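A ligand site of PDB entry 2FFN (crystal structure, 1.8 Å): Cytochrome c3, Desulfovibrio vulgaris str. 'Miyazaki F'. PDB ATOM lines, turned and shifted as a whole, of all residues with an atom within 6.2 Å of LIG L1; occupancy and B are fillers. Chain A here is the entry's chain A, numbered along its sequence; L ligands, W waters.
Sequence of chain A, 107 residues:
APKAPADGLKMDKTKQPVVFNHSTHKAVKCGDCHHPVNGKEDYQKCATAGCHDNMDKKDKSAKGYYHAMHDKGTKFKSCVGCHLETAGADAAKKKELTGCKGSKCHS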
ATOM      1  N   MET A  11       8.912  13.959  -8.837  1.00  0.00           N
ATOM      2  CA  MET A  11       8.989  15.413  -8.982  1.00  0.00           C
ATOM      3  C   MET A  11       8.217  15.749 -10.239  1.00  0.00           C
ATOM      4  O   MET A  11       8.599  15.338 -11.341  1.00  0.00           O
ATOM      5  CB  MET A  11      10.446  15.847  -9.121  1.00  0.00           C
ATOM      6  CG  MET A  11      11.317  15.351  -7.962  1.00  0.00           C
ATOM      7  SD  MET A  11      13.101  15.596  -8.127  1.00  0.00           S
ATOM      8  CE  MET A  11      13.272  17.354  -7.880  1.00  0.00           C
ATOM      9  N   ASP A  12       7.114  16.467 -10.088  1.00  0.00           N
ATOM     10  CA  ASP A  12       6.220  16.713 -11.214  1.00  0.00           C
ATOM     11  C   ASP A  12       5.704  18.142 -11.261  1.00  0.00           C
ATOM     12  O   ASP A  12       4.509  18.373 -11.466  1.00  0.00           O
ATOM     13  CB  ASP A  12       5.042  15.729 -11.185  1.00  0.00           C
ATOM     14  CG  ASP A  12       4.356  15.655  -9.839  1.00  0.00           C
ATOM     15  OD1 ASP A  12       4.487  16.605  -9.036  1.00  0.00           O
ATOM     16  OD2 ASP A  12       3.679  14.640  -9.581  1.00  0.00           O
ATOM     17  N   LYS A  13       6.605  19.095 -11.079  1.00  0.00           N
ATOM     18  CA  LYS A  13       6.262  20.500 -11.238  1.00  0.00           C
ATOM     19  C   LYS A  13       6.132  20.855 -12.718  1.00  0.00           C
ATOM     20  O   LYS A  13       5.528  21.870 -13.071  1.00  0.00           O
ATOM     21  CB  LYS A  13       7.342  21.371 -10.594  1.00  0.00           C
ATOM     22  CG  LYS A  13       7.632  21.029  -9.144  1.00  0.00           C
ATOM     23  CD  LYS A  13       6.856  21.914  -8.177  1.00  0.00           C
ATOM     24  CE  LYS A  13       5.399  21.499  -8.066  1.00  0.00           C
ATOM     25  NZ  LYS A  13       4.701  22.298  -7.006  1.00  0.00           N
ATOM     26  N   THR A  14       6.694  20.013 -13.579  1.00  0.00           N
ATOM     27  CA  THR A  14       6.801  20.328 -15.003  1.00  0.00           C
ATOM     28  C   THR A  14       6.181  19.211 -15.842  1.00  0.00           C
ATOM     29  O   THR A  14       5.689  18.217 -15.296  1.00  0.00           O
ATOM     30  CB  THR A  14       8.273  20.468 -15.440  1.00  0.00           C
ATOM     31  OG1 THR A  14       8.879  19.168 -15.504  1.00  0.00           O
ATOM     32  CG2 THR A  14       9.037  21.325 -14.419  1.00  0.00           C
ATOM     33  N   LYS A  15       6.207  19.374 -17.157  1.00  0.00           N
ATOM     34  CA  LYS A  15       5.673  18.348 -18.042  1.00  0.00           C
ATOM     35  C   LYS A  15       6.685  17.244 -18.348  1.00  0.00           C
ATOM     36  O   LYS A  15       6.377  16.297 -19.074  1.00  0.00           O
ATOM     37  CB  LYS A  15       5.164  18.992 -19.342  1.00  0.00           C
ATOM     38  CG  LYS A  15       4.002  19.932 -19.115  1.00  0.00           C
ATOM     39  CD  LYS A  15       3.385  20.395 -20.416  1.00  0.00           C
ATOM     40  CE  LYS A  15       2.173  21.265 -20.172  1.00  0.00           C
ATOM     41  NZ  LYS A  15       1.484  21.592 -21.445  1.00  0.00           N
ATOM     42  N   GLN A  16       7.882  17.356 -17.783  1.00  0.00           N
ATOM     43  CA  GLN A  16       8.878  16.295 -17.878  1.00  0.00           C
ATOM     44  C   GLN A  16       9.197  15.813 -16.456  1.00  0.00           C
ATOM     45  O   GLN A  16      10.301  16.015 -15.945  1.00  0.00           O
ATOM     46  CB  GLN A  16      10.158  16.808 -18.538  1.00  0.00           C
ATOM     47  CG  GLN A  16       9.936  17.572 -19.842  1.00  0.00           C
ATOM     48  CD  GLN A  16       9.328  16.708 -20.929  1.00  0.00           C
ATOM     49  OE1 GLN A  16       9.533  15.500 -20.960  1.00  0.00           O
ATOM     50  NE2 GLN A  16       8.567  17.334 -21.821  1.00  0.00           N
ATOM     51  N   PRO A  17       8.239  15.144 -15.806  1.00  0.00           N
ATOM     52  CA  PRO A  17       8.431  14.636 -14.439  1.00  0.00           C
ATOM     53  C   PRO A  17       9.535  13.592 -14.295  1.00  0.00           C
ATOM     54  O   PRO A  17       9.784  12.818 -15.220  1.00  0.00           O
ATOM     55  CB  PRO A  17       7.050  14.062 -14.077  1.00  0.00           C
ATOM     56  CG  PRO A  17       6.454  13.688 -15.396  1.00  0.00           C
ATOM     57  CD  PRO A  17       6.945  14.715 -16.374  1.00  0.00           C
ATOM     58  N   VAL A  18      10.182  13.588 -13.137  1.00  0.00           N
ATOM     59  CA  VAL A  18      11.312  12.708 -12.861  1.00  0.00           C
ATOM     60  C   VAL A  18      11.121  12.051 -11.500  1.00  0.00           C
ATOM     61  O   VAL A  18      10.645  12.692 -10.554  1.00  0.00           O
ATOM     62  CB  VAL A  18      12.638  13.515 -12.868  1.00  0.00           C
ATOM     63  CG1 VAL A  18      13.816  12.593 -12.601  1.00  0.00           C
ATOM     64  CG2 VAL A  18      12.798  14.232 -14.201  1.00  0.00           C
ATOM     65  N   MET A  55       9.263  28.816 -12.522  1.00  0.00           N
ATOM     66  CA  MET A  55       9.157  27.750 -13.516  1.00  0.00           C
ATOM     67  C   MET A  55       9.557  28.204 -14.931  1.00  0.00           C
ATOM     68  O   MET A  55       9.236  27.536 -15.913  1.00  0.00           O
ATOM     69  CB  MET A  55       7.734  27.189 -13.549  1.00  0.00           C
ATOM     70  CG  MET A  55       7.319  26.444 -12.282  1.00  0.00           C
ATOM     71  SD  MET A  55       8.360  24.980 -11.990  1.00  0.00           S
ATOM     72  CE  MET A  55       8.467  24.971 -10.203  1.00  0.00           C
ATOM     73  N   ASP A  56      10.244  29.338 -15.011  1.00  0.00           N
ATOM     74  CA  ASP A  56      10.869  29.768 -16.259  1.00  0.00           C
ATOM     75  C   ASP A  56      12.206  29.029 -16.397  1.00  0.00           C
ATOM     76  O   ASP A  56      13.165  29.345 -15.701  1.00  0.00           O
ATOM     77  CB  ASP A  56      11.122  31.283 -16.214  1.00  0.00           C
ATOM     78  CG  ASP A  56      11.893  31.805 -17.432  1.00  0.00           C
ATOM     79  OD1 ASP A  56      12.261  32.994 -17.431  1.00  0.00           O
ATOM     80  OD2 ASP A  56      12.131  31.033 -18.377  1.00  0.00           O
ATOM     81  N   LYS A  57      12.258  28.064 -17.306  1.00  0.00           N
ATOM     82  CA  LYS A  57      13.417  27.171 -17.410  1.00  0.00           C
ATOM     83  C   LYS A  57      14.679  27.880 -17.901  1.00  0.00           C
ATOM     84  O   LYS A  57      15.757  27.287 -17.911  1.00  0.00           O
ATOM     85  CB  LYS A  57      13.097  25.983 -18.328  1.00  0.00           C
ATOM     86  CG  LYS A  57      12.973  26.327 -19.801  1.00  0.00           C
ATOM     87  CD  LYS A  57      12.780  25.053 -20.606  1.00  0.00           C
ATOM     88  CE  LYS A  57      12.640  25.339 -22.091  1.00  0.00           C
ATOM     89  NZ  LYS A  57      12.241  24.104 -22.821  1.00  0.00           N
ATOM     90  N   TYR A  65      13.838  26.904 -10.955  1.00  0.00           N
ATOM     91  CA  TYR A  65      13.672  25.486 -10.657  1.00  0.00           C
ATOM     92  C   TYR A  65      14.527  24.626 -11.589  1.00  0.00           C
ATOM     93  O   TYR A  65      15.282  23.767 -11.141  1.00  0.00           O
ATOM     94  CB  TYR A  65      12.190  25.109 -10.765  1.00  0.00           C
ATOM     95  CG  TYR A  65      11.867  23.678 -10.422  1.00  0.00           C
ATOM     96  CD1 TYR A  65      11.619  22.737 -11.426  1.00  0.00           C
ATOM     97  CD2 TYR A  65      11.760  23.257  -9.099  1.00  0.00           C
ATOM     98  CE1 TYR A  65      11.293  21.418 -11.119  1.00  0.00           C
ATOM     99  CE2 TYR A  65      11.438  21.938  -8.779  1.00  0.00           C
ATOM    100  CZ  TYR A  65      11.188  21.027  -9.789  1.00  0.00           C
ATOM    101  OH  TYR A  65      10.867  19.728  -9.483  1.00  0.00           O
ATOM    102  N   TYR A  66      14.424  24.860 -12.893  1.00  0.00           N
ATOM    103  CA  TYR A  66      15.191  24.110 -13.880  1.00  0.00           C
ATOM    104  C   TYR A  66      16.687  24.255 -13.610  1.00  0.00           C
ATOM    105  O   TYR A  66      17.443  23.281 -13.673  1.00  0.00           O
ATOM    106  CB  TYR A  66      14.871  24.614 -15.295  1.00  0.00           C
ATOM    107  CG  TYR A  66      15.658  23.906 -16.387  1.00  0.00           C
ATOM    108  CD1 TYR A  66      16.972  24.254 -16.665  1.00  0.00           C
ATOM    109  CD2 TYR A  66      15.068  22.869 -17.124  1.00  0.00           C
ATOM    110  CE1 TYR A  66      17.701  23.584 -17.645  1.00  0.00           C
ATOM    111  CE2 TYR A  66      15.795  22.190 -18.103  1.00  0.00           C
ATOM    112  CZ  TYR A  66      17.102  22.560 -18.366  1.00  0.00           C
ATOM    113  OH  TYR A  66      17.820  21.894 -19.329  1.00  0.00           O
ATOM    114  N   MET A  69      18.259  22.159 -10.899  1.00  0.00           N
ATOM    115  CA  MET A  69      18.225  20.727 -11.215  1.00  0.00           C
ATOM    116  C   MET A  69      19.253  20.344 -12.295  1.00  0.00           C
ATOM    117  O   MET A  69      19.645  19.164 -12.391  1.00  0.00           O
ATOM    118  CB  MET A  69      16.827  20.345 -11.692  1.00  0.00           C
ATOM    119  CG  MET A  69      15.975  19.523 -10.724  1.00  0.00           C
ATOM    120  SD  MET A  69      16.176  19.841  -8.963  1.00  0.00           S
ATOM    121  CE  MET A  69      14.940  21.150  -8.650  1.00  0.00           C
ATOM    122  N   HIS A  70      19.672  21.302 -13.102  1.00  0.00           N
ATOM    123  CA  HIS A  70      20.411  20.979 -14.336  1.00  0.00           C
ATOM    124  C   HIS A  70      21.800  21.602 -14.484  1.00  0.00           C
ATOM    125  O   HIS A  70      22.642  21.052 -15.204  1.00  0.00           O
ATOM    126  CB  HIS A  70      19.591  21.368 -15.562  1.00  0.00           C
ATOM    127  CG  HIS A  70      18.355  20.542 -15.760  1.00  0.00           C
ATOM    128  ND1 HIS A  70      17.166  20.868 -15.153  1.00  0.00           N
ATOM    129  CD2 HIS A  70      18.136  19.422 -16.466  1.00  0.00           C
ATOM    130  CE1 HIS A  70      16.249  19.973 -15.490  1.00  0.00           C
ATOM    131  NE2 HIS A  70      16.819  19.081 -16.289  1.00  0.00           N
ATOM    132  N   CYS A  79      21.356  18.019  -9.735  1.00  0.00           N
ATOM    133  CA  CYS A  79      21.168  16.673 -10.267  1.00  0.00           C
ATOM    134  C   CYS A  79      22.216  16.379 -11.351  1.00  0.00           C
ATOM    135  O   CYS A  79      23.038  15.470 -11.226  1.00  0.00           O
ATOM    136  CB  CYS A  79      19.771  16.501 -10.881  1.00  0.00           C
ATOM    137  SG  CYS A  79      18.370  16.908  -9.773  1.00  0.00           S
ATOM    138  N   VAL A  80      22.166  17.155 -12.421  1.00  0.00           N
ATOM    139  CA  VAL A  80      23.018  16.871 -13.576  1.00  0.00           C
ATOM    140  C   VAL A  80      24.476  17.142 -13.197  1.00  0.00           C
ATOM    141  O   VAL A  80      25.387  16.405 -13.593  1.00  0.00           O
ATOM    142  CB  VAL A  80      22.657  17.731 -14.796  1.00  0.00           C
ATOM    143  CG1 VAL A  80      23.562  17.404 -15.967  1.00  0.00           C
ATOM    144  CG2 VAL A  80      21.191  17.461 -15.180  1.00  0.00           C
ATOM    145  N   HIS A  83      25.897  14.276 -11.263  1.00  0.00           N
ATOM    146  CA  HIS A  83      25.917  13.106 -12.130  1.00  0.00           C
ATOM    147  C   HIS A  83      27.024  13.190 -13.174  1.00  0.00           C
ATOM    148  O   HIS A  83      27.625  12.166 -13.526  1.00  0.00           O
ATOM    149  CB  HIS A  83      24.557  12.942 -12.829  1.00  0.00           C
ATOM    150  CG  HIS A  83      23.488  12.361 -11.943  1.00  0.00           C
ATOM    151  ND1 HIS A  83      22.301  11.869 -12.452  1.00  0.00           N
ATOM    152  CD2 HIS A  83      23.427  12.196 -10.615  1.00  0.00           C
ATOM    153  CE1 HIS A  83      21.559  11.423 -11.448  1.00  0.00           C
ATOM    154  NE2 HIS A  83      22.216  11.611 -10.320  1.00  0.00           N
ATOM    155  N   GLU A  96      23.235   7.482 -19.285  1.00  0.00           N
ATOM    156  CA  GLU A  96      22.314   7.028 -18.239  1.00  0.00           C
ATOM    157  C   GLU A  96      22.002   8.108 -17.209  1.00  0.00           C
ATOM    158  O   GLU A  96      20.875   8.199 -16.722  1.00  0.00           O
ATOM    159  CB  GLU A  96      22.876   5.814 -17.511  1.00  0.00           C
ATOM    160  CG  GLU A  96      22.971   4.565 -18.349  1.00  0.00           C
ATOM    161  CD  GLU A  96      23.518   3.388 -17.552  1.00  0.00           C
ATOM    162  OE1 GLU A  96      23.734   3.546 -16.334  1.00  0.00           O
ATOM    163  OE2 GLU A  96      23.721   2.321 -18.159  1.00  0.00           O
ATOM    164  N   LEU A  97      23.015   8.890 -16.847  1.00  0.00           N
ATOM    165  CA  LEU A  97      22.915   9.773 -15.698  1.00  0.00           C
ATOM    166  C   LEU A  97      22.794  11.252 -16.065  1.00  0.00           C
ATOM    167  O   LEU A  97      22.322  12.050 -15.256  1.00  0.00           O
ATOM    168  CB  LEU A  97      24.105   9.554 -14.758  1.00  0.00           C
ATOM    169  CG  LEU A  97      24.230   8.156 -14.162  1.00  0.00           C
ATOM    170  CD1 LEU A  97      25.500   8.069 -13.316  1.00  0.00           C
ATOM    171  CD2 LEU A  97      23.007   7.833 -13.319  1.00  0.00           C
ATOM    172  N   THR A  98      23.213  11.628 -17.281  1.00  0.00           N
ATOM    173  CA  THR A  98      23.134  13.024 -17.677  1.00  0.00           C
ATOM    174  C   THR A  98      22.403  13.276 -19.000  1.00  0.00           C
ATOM    175  O   THR A  98      22.210  14.432 -19.388  1.00  0.00           O
ATOM    176  CB  THR A  98      24.545  13.675 -17.779  1.00  0.00           C
ATOM    177  OG1 THR A  98      25.254  13.128 -18.892  1.00  0.00           O
ATOM    178  CG2 THR A  98      25.330  13.409 -16.502  1.00  0.00           C
ATOM    179  N   GLY A  99      21.983  12.213 -19.668  1.00  0.00           N
ATOM    180  CA  GLY A  99      21.316  12.360 -20.952  1.00  0.00           C
ATOM    181  C   GLY A  99      20.009  13.111 -20.871  1.00  0.00           C
ATOM    182  O   GLY A  99      19.237  12.958 -19.918  1.00  0.00           O
ATOM    183  N   CYS A 100      19.739  13.940 -21.878  1.00  0.00           N
ATOM    184  CA  CYS A 100      18.516  14.738 -21.920  1.00  0.00           C
ATOM    185  C   CYS A 100      17.327  13.901 -22.363  1.00  0.00           C
ATOM    186  O   CYS A 100      16.174  14.265 -22.116  1.00  0.00           O
ATOM    187  CB  CYS A 100      18.707  15.927 -22.849  1.00  0.00           C
ATOM    188  SG  CYS A 100      20.101  17.016 -22.415  1.00  0.00           S
ATOM    189  N   LYS A 101      17.604  12.793 -23.035  1.00  0.00           N
ATOM    190  CA  LYS A 101      16.591  11.807 -23.382  1.00  0.00           C
ATOM    191  C   LYS A 101      17.182  10.417 -23.220  1.00  0.00           C
ATOM    192  O   LYS A 101      18.397  10.245 -23.220  1.00  0.00           O
ATOM    193  CB  LYS A 101      16.134  12.001 -24.828  1.00  0.00           C
ATOM    194  CG  LYS A 101      17.268  11.896 -25.842  1.00  0.00           C
ATOM    195  CD  LYS A 101      16.759  12.011 -27.271  1.00  0.00           C
ATOM    196  CE  LYS A 101      15.941  10.794 -27.663  1.00  0.00           C
ATOM    197  NZ  LYS A 101      15.388  10.931 -29.041  1.00  0.00           N
ATOM    198  N   SER A 103      17.521   8.662 -20.736  1.00  0.00           N
ATOM    199  CA  SER A 103      18.309   8.547 -19.511  1.00  0.00           C
ATOM    200  C   SER A 103      17.432   8.067 -18.358  1.00  0.00           C
ATOM    201  O   SER A 103      16.215   7.915 -18.516  1.00  0.00           O
ATOM    202  CB  SER A 103      18.925   9.901 -19.146  1.00  0.00           C
ATOM    203  OG  SER A 103      17.929  10.840 -18.784  1.00  0.00           O
ATOM    204  N   LYS A 104      18.053   7.832 -17.209  1.00  0.00           N
ATOM    205  CA  LYS A 104      17.324   7.392 -16.028  1.00  0.00           C
ATOM    206  C   LYS A 104      16.449   8.507 -15.474  1.00  0.00           C
ATOM    207  O   LYS A 104      15.565   8.260 -14.651  1.00  0.00           O
ATOM    208  CB  LYS A 104      18.294   6.911 -14.952  1.00  0.00           C
ATOM    209  CG  LYS A 104      19.201   5.772 -15.418  1.00  0.00           C
ATOM    210  CD  LYS A 104      19.260   4.654 -14.385  1.00  0.00           C
ATOM    211  CE  LYS A 104      19.881   3.400 -14.970  1.00  0.00           C
ATOM    212  NZ  LYS A 104      18.973   2.702 -15.935  1.00  0.00           N
ATOM    213  N   CYS A 105      16.678   9.739 -15.913  1.00  0.00           N
ATOM    214  CA  CYS A 105      15.828  10.853 -15.501  1.00  0.00           C
ATOM    215  C   CYS A 105      14.697  11.128 -16.474  1.00  0.00           C
ATOM    216  O   CYS A 105      13.541  11.254 -16.061  1.00  0.00           O
ATOM    217  CB  CYS A 105      16.646  12.132 -15.339  1.00  0.00           C
ATOM    218  SG  CYS A 105      17.874  12.096 -13.996  1.00  0.00           S
ATOM    219  N   HIS A 106      15.029  11.254 -17.760  1.00  0.00           N
ATOM    220  CA  HIS A 106      14.029  11.529 -18.780  1.00  0.00           C
ATOM    221  C   HIS A 106      13.940  10.387 -19.785  1.00  0.00           C
ATOM    222  O   HIS A 106      14.933  10.032 -20.419  1.00  0.00           O
ATOM    223  CB  HIS A 106      14.367  12.825 -19.536  1.00  0.00           C
ATOM    224  CG  HIS A 106      14.345  14.058 -18.683  1.00  0.00           C
ATOM    225  ND1 HIS A 106      13.238  14.452 -17.962  1.00  0.00           N
ATOM    226  CD2 HIS A 106      15.297  15.001 -18.453  1.00  0.00           C
ATOM    227  CE1 HIS A 106      13.505  15.579 -17.322  1.00  0.00           C
ATOM    228  NE2 HIS A 106      14.752  15.931 -17.609  1.00  0.00           N
HETATM  229  C1  LIG L   1      12.806  18.876 -15.931  1.00  0.00           C
HETATM  230  C2  LIG L   1      15.385  19.092 -19.975  1.00  0.00           C
HETATM  231  C3  LIG L   1      18.601  16.094 -18.115  1.00  0.00           C
HETATM  232  C4  LIG L   1      16.160  16.067 -13.968  1.00  0.00           C
HETATM  233  C5  LIG L   1      13.108  19.149 -17.291  1.00  0.00           C
HETATM  234  C6  LIG L   1      12.374  19.881 -18.211  1.00  0.00           C
HETATM  235  C7  LIG L   1      13.115  19.920 -19.380  1.00  0.00           C
HETATM  236  C8  LIG L   1      14.282  19.226 -19.104  1.00  0.00           C
HETATM  237  C9  LIG L   1      12.753  20.581 -20.708  1.00  0.00           C
HETATM  238  C10 LIG L   1      11.050  20.580 -17.996  1.00  0.00           C
HETATM  239  C11 LIG L   1      11.235  22.069 -17.736  1.00  0.00           C
HETATM  240  C12 LIG L   1       9.922  22.818 -17.718  1.00  0.00           C
HETATM  241  O1  LIG L   1       9.106  22.645 -18.650  1.00  0.00           O
HETATM  242  O2  LIG L   1       9.700  23.587 -16.762  1.00  0.00           O
HETATM  243  C13 LIG L   1      16.600  18.415 -19.781  1.00  0.00           C
HETATM  244  C14 LIG L   1      17.684  18.471 -20.641  1.00  0.00           C
HETATM  245  C15 LIG L   1      18.639  17.600 -20.131  1.00  0.00           C
HETATM  246  C16 LIG L   1      18.060  17.062 -18.977  1.00  0.00           C
HETATM  247  C17 LIG L   1      17.814  19.394 -21.875  1.00  0.00           C
HETATM  248  C18 LIG L   1      19.918  17.311 -20.588  1.00  0.00           C
HETATM  249  C19 LIG L   1      20.825  18.346 -21.099  1.00  0.00           C
HETATM  250  C20 LIG L   1      18.178  15.692 -16.811  1.00  0.00           C
HETATM  251  C21 LIG L   1      18.763  14.722 -16.029  1.00  0.00           C
HETATM  252  C22 LIG L   1      18.049  14.688 -14.843  1.00  0.00           C
HETATM  253  C23 LIG L   1      17.079  15.673 -14.948  1.00  0.00           C
HETATM  254  C24 LIG L   1      19.917  13.835 -16.478  1.00  0.00           C
HETATM  255  C25 LIG L   1      18.245  13.882 -13.707  1.00  0.00           C
HETATM  256  C26 LIG L   1      19.569  13.480 -13.238  1.00  0.00           C
HETATM  257  C27 LIG L   1      15.066  16.948 -14.049  1.00  0.00           C
HETATM  258  C28 LIG L   1      14.223  17.275 -13.018  1.00  0.00           C
HETATM  259  C29 LIG L   1      13.194  18.006 -13.623  1.00  0.00           C
HETATM  260  C30 LIG L   1      13.541  18.167 -14.955  1.00  0.00           C
HETATM  261  C31 LIG L   1      14.320  16.897 -11.532  1.00  0.00           C
HETATM  262  C32 LIG L   1      11.949  18.543 -12.948  1.00  0.00           C
HETATM  263  C33 LIG L   1      10.835  17.514 -12.916  1.00  0.00           C
HETATM  264  C34 LIG L   1       9.499  18.110 -12.520  1.00  0.00           C
HETATM  265  O3  LIG L   1       9.422  18.689 -11.418  1.00  0.00           O
HETATM  266  O4  LIG L   1       8.527  17.999 -13.300  1.00  0.00           O
HETATM  267  N1  LIG L   1      14.217  18.719 -17.883  1.00  0.00           N
HETATM  268  N2  LIG L   1      16.886  17.645 -18.762  1.00  0.00           N
HETATM  269  N3  LIG L   1      17.159  16.239 -16.158  1.00  0.00           N
HETATM  270  N4  LIG L   1      14.695  17.558 -15.166  1.00  0.00           N
HETATM  271 FE1  LIG L   1      15.742  17.550 -16.998  1.00  0.00          FE
HETATM  272  C1  LG2 L   2      21.813   7.872  -9.415  1.00  0.00           C
HETATM  273  C2  LG2 L   2      18.319  11.108 -10.071  1.00  0.00           C
HETATM  274  C3  LG2 L   2      20.910  14.362  -7.634  1.00  0.00           C
HETATM  275  C4  LG2 L   2      24.482  11.182  -7.180  1.00  0.00           C
HETATM  276  C5  LG2 L   2      20.588   8.439  -9.838  1.00  0.00           C
HETATM  277  C6  LG2 L   2      19.624   7.784 -10.569  1.00  0.00           C
HETATM  278  C7  LG2 L   2      18.603   8.715 -10.757  1.00  0.00           C
HETATM  279  C8  LG2 L   2      19.024   9.879 -10.132  1.00  0.00           C
HETATM  280  C9  LG2 L   2      17.282   8.510 -11.508  1.00  0.00           C
HETATM  281  C10 LG2 L   2      19.700   6.341 -11.029  1.00  0.00           C
HETATM  282  C11 LG2 L   2      19.259   5.368  -9.967  1.00  0.00           C
HETATM  283  C12 LG2 L   2      17.802   5.541  -9.568  1.00  0.00           C
HETATM  284  O1  LG2 L   2      16.921   5.232 -10.409  1.00  0.00           O
HETATM  285  O2  LG2 L   2      17.541   5.998  -8.432  1.00  0.00           O
HETATM  286  C13 LG2 L   2      18.678  12.346  -9.477  1.00  0.00           C
HETATM  287  C14 LG2 L   2      17.918  13.513  -9.478  1.00  0.00           C
HETATM  288  C15 LG2 L   2      18.648  14.457  -8.739  1.00  0.00           C
HETATM  289  C16 LG2 L   2      19.839  13.824  -8.374  1.00  0.00           C
HETATM  290  C17 LG2 L   2      16.566  13.625 -10.165  1.00  0.00           C
HETATM  291  C18 LG2 L   2      18.287  15.756  -8.354  1.00  0.00           C
HETATM  292  C19 LG2 L   2      16.896  16.192  -8.170  1.00  0.00           C
HETATM  293  C20 LG2 L   2      22.163  13.826  -7.296  1.00  0.00           C
HETATM  294  C21 LG2 L   2      23.210  14.490  -6.645  1.00  0.00           C
HETATM  295  C22 LG2 L   2      24.258  13.578  -6.577  1.00  0.00           C
HETATM  296  C23 LG2 L   2      23.789  12.389  -7.106  1.00  0.00           C
HETATM  297  C24 LG2 L   2      23.106  15.949  -6.194  1.00  0.00           C
HETATM  298  C25 LG2 L   2      25.545  13.749  -6.072  1.00  0.00           C
HETATM  299  C26 LG2 L   2      25.934  14.916  -5.311  1.00  0.00           C
HETATM  300  C27 LG2 L   2      24.101   9.960  -7.755  1.00  0.00           C
HETATM  301  C28 LG2 L   2      24.853   8.804  -7.774  1.00  0.00           C
HETATM  302  C29 LG2 L   2      24.074   7.855  -8.411  1.00  0.00           C
HETATM  303  C30 LG2 L   2      22.897   8.476  -8.764  1.00  0.00           C
HETATM  304  C31 LG2 L   2      26.262   8.632  -7.221  1.00  0.00           C
HETATM  305  C32 LG2 L   2      24.436   6.415  -8.731  1.00  0.00           C
HETATM  306  C33 LG2 L   2      25.346   6.321  -9.933  1.00  0.00           C
HETATM  307  C34 LG2 L   2      25.048   5.119 -10.797  1.00  0.00           C
HETATM  308  O3  LG2 L   2      25.855   4.816 -11.698  1.00  0.00           O
HETATM  309  O4  LG2 L   2      24.000   4.473 -10.577  1.00  0.00           O
HETATM  310  N1  LG2 L   2      20.211   9.685  -9.587  1.00  0.00           N
HETATM  311  N2  LG2 L   2      19.813  12.568  -8.829  1.00  0.00           N
HETATM  312  N3  LG2 L   2      22.527  12.572  -7.566  1.00  0.00           N
HETATM  313  N4  LG2 L   2      22.942   9.744  -8.384  1.00  0.00           N
HETATM  314 FE1  LG2 L   2      21.371  11.148  -8.591  1.00  0.00          FE
HETATM  315  O   HOH W   1       6.561  22.030 -18.420  1.00  0.00           O
HETATM  316  O   HOH W   2       7.684  25.186 -16.208  1.00  0.00           O
HETATM  317  O   HOH W   3      10.943  24.466 -14.602  1.00  0.00           O
HETATM  318  O   HOH W   4      14.593  22.615 -22.871  1.00  0.00           O
HETATM  319  O   HOH W   5      13.154  16.710 -20.775  1.00  0.00           O
HETATM  320  O   HOH W   6       9.776  22.631 -21.145  1.00  0.00           O
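SG of Cys 105 is covalently linked to C25 of LIG L1 (1.8 Å). The side-chain sulfur of Cys 100 is covalently linked to a carbon (C18) of LIG L1 (1.9 Å). NE2 of His 106 binds FE1 of LIG L1 (2.0 Å). A ring nitrogen (NE2) of His 70 binds an iron atom (FE1) of LIG L1 (2.0 Å). An oxygen (O4) of LIG L1 lies within hydrogen-bond range of the backbone NH of Thr 14, at 2.7 Å. OG1 of Thr 14 is in hydrogen-bond range of O4 of LIG L1. The side-chain hydroxyl of Tyr 65 is in hydrogen-bond range of an oxygen (O3) of LIG L1 (2.6 Å). The backbone NH (N) of Lys 13 is in hydrogen-bond range of an oxygen (O3) of LIG L1. The backbone NH (N) of Asp 12 is in hydrogen-bond range of an oxygen (O3) of LIG L1 (3.5 Å). FE1 of LG2 L2 is bound by NE2 of His 83 (2.0 Å). SG of Cys 79 is covalently linked to C18 of LG2 L2, at 1.8 Å.
Water W6 bridges an oxygen (O1) of LIG L1 (2.6 Å) and the side-chain amino group (NZ) of Lys 57 (3.3 Å). Water W1 lies within hydrogen-bond range of O1 of LIG L1 and N of Lys 15. Water W2 lies within hydrogen-bond range of an oxygen (O2) of LIG L1 and the backbone carbonyl oxygen (O) of Met 55. Water W3 bridges O2 of LIG L1 (2.6 Å) and SD of Met 55 (3.7 Å).
The side-chain hydroxyl of Ser 103 sits close to the backbone NH of Cys 105 (3.3 Å). The side-chain hydroxyl of Ser 103 lies within hydrogen-bond range of the backbone NH of His 106 (3.1 Å). ND1 of His 70 is in hydrogen-bond range of O of Tyr 66, 2.8 Å away. The side-chain hydroxyl (OG1) of Thr 14 sits at hydrogen-bond distance from the backbone NH (N) of Gln 16, 3.1 Å away. The backbone NH of Met 11 lies within hydrogen-bond range of the backbone carbonyl oxygen of Val 18 (2.7 Å). N of Val 80 lies within hydrogen-bond range of O of Met 69, 3.2 Å away. The backbone carbonyl oxygen of Leu 97 sits at hydrogen-bond distance from a ring nitrogen (ND1) of His 83, at 2.8 Å. O of Gly 99 lies within hydrogen-bond range of OG of Ser 103, 2.7 Å away.
An oxygen (O4) of LIG L1 sits close to the backbone carbonyl oxygen of Met 11 (3.3 Å). Gln 16 touches LIG L1 (O to C33, 3.4 Å). CA of Pro 17 touches O4 of LIG L1, at 3.6 Å. Val 18 touches LIG L1. Tyr 66 touches LIG L1 (CE2 to C8, 3.5 Å). CG of Met 69 touches C31 of LIG L1, 3.2 Å away. CB of Cys 79 touches C26 of LIG L1 (3.8 Å). Val 80 touches LIG L1. His 83 touches LIG L1 (ND1 to C26, 3.3 Å). O of Leu 97 touches C24 of LIG L1, at 3.2 Å. Thr 98 touches LIG L1 (CA to C24, 3.5 Å). Gly 99 touches LIG L1. Hydrophobic or aromatic side chains within 4 Å of LIG L1: Met 11, Val 18, Tyr 65, Tyr 66, Met 69, His 70, Val 80, His 83 and His 106. Of the 28 residues printed, 20 come within 4 Å of LIG L1. The nearest printed residue that does not touch LIG L1 is Met 55 (4.1 Å).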
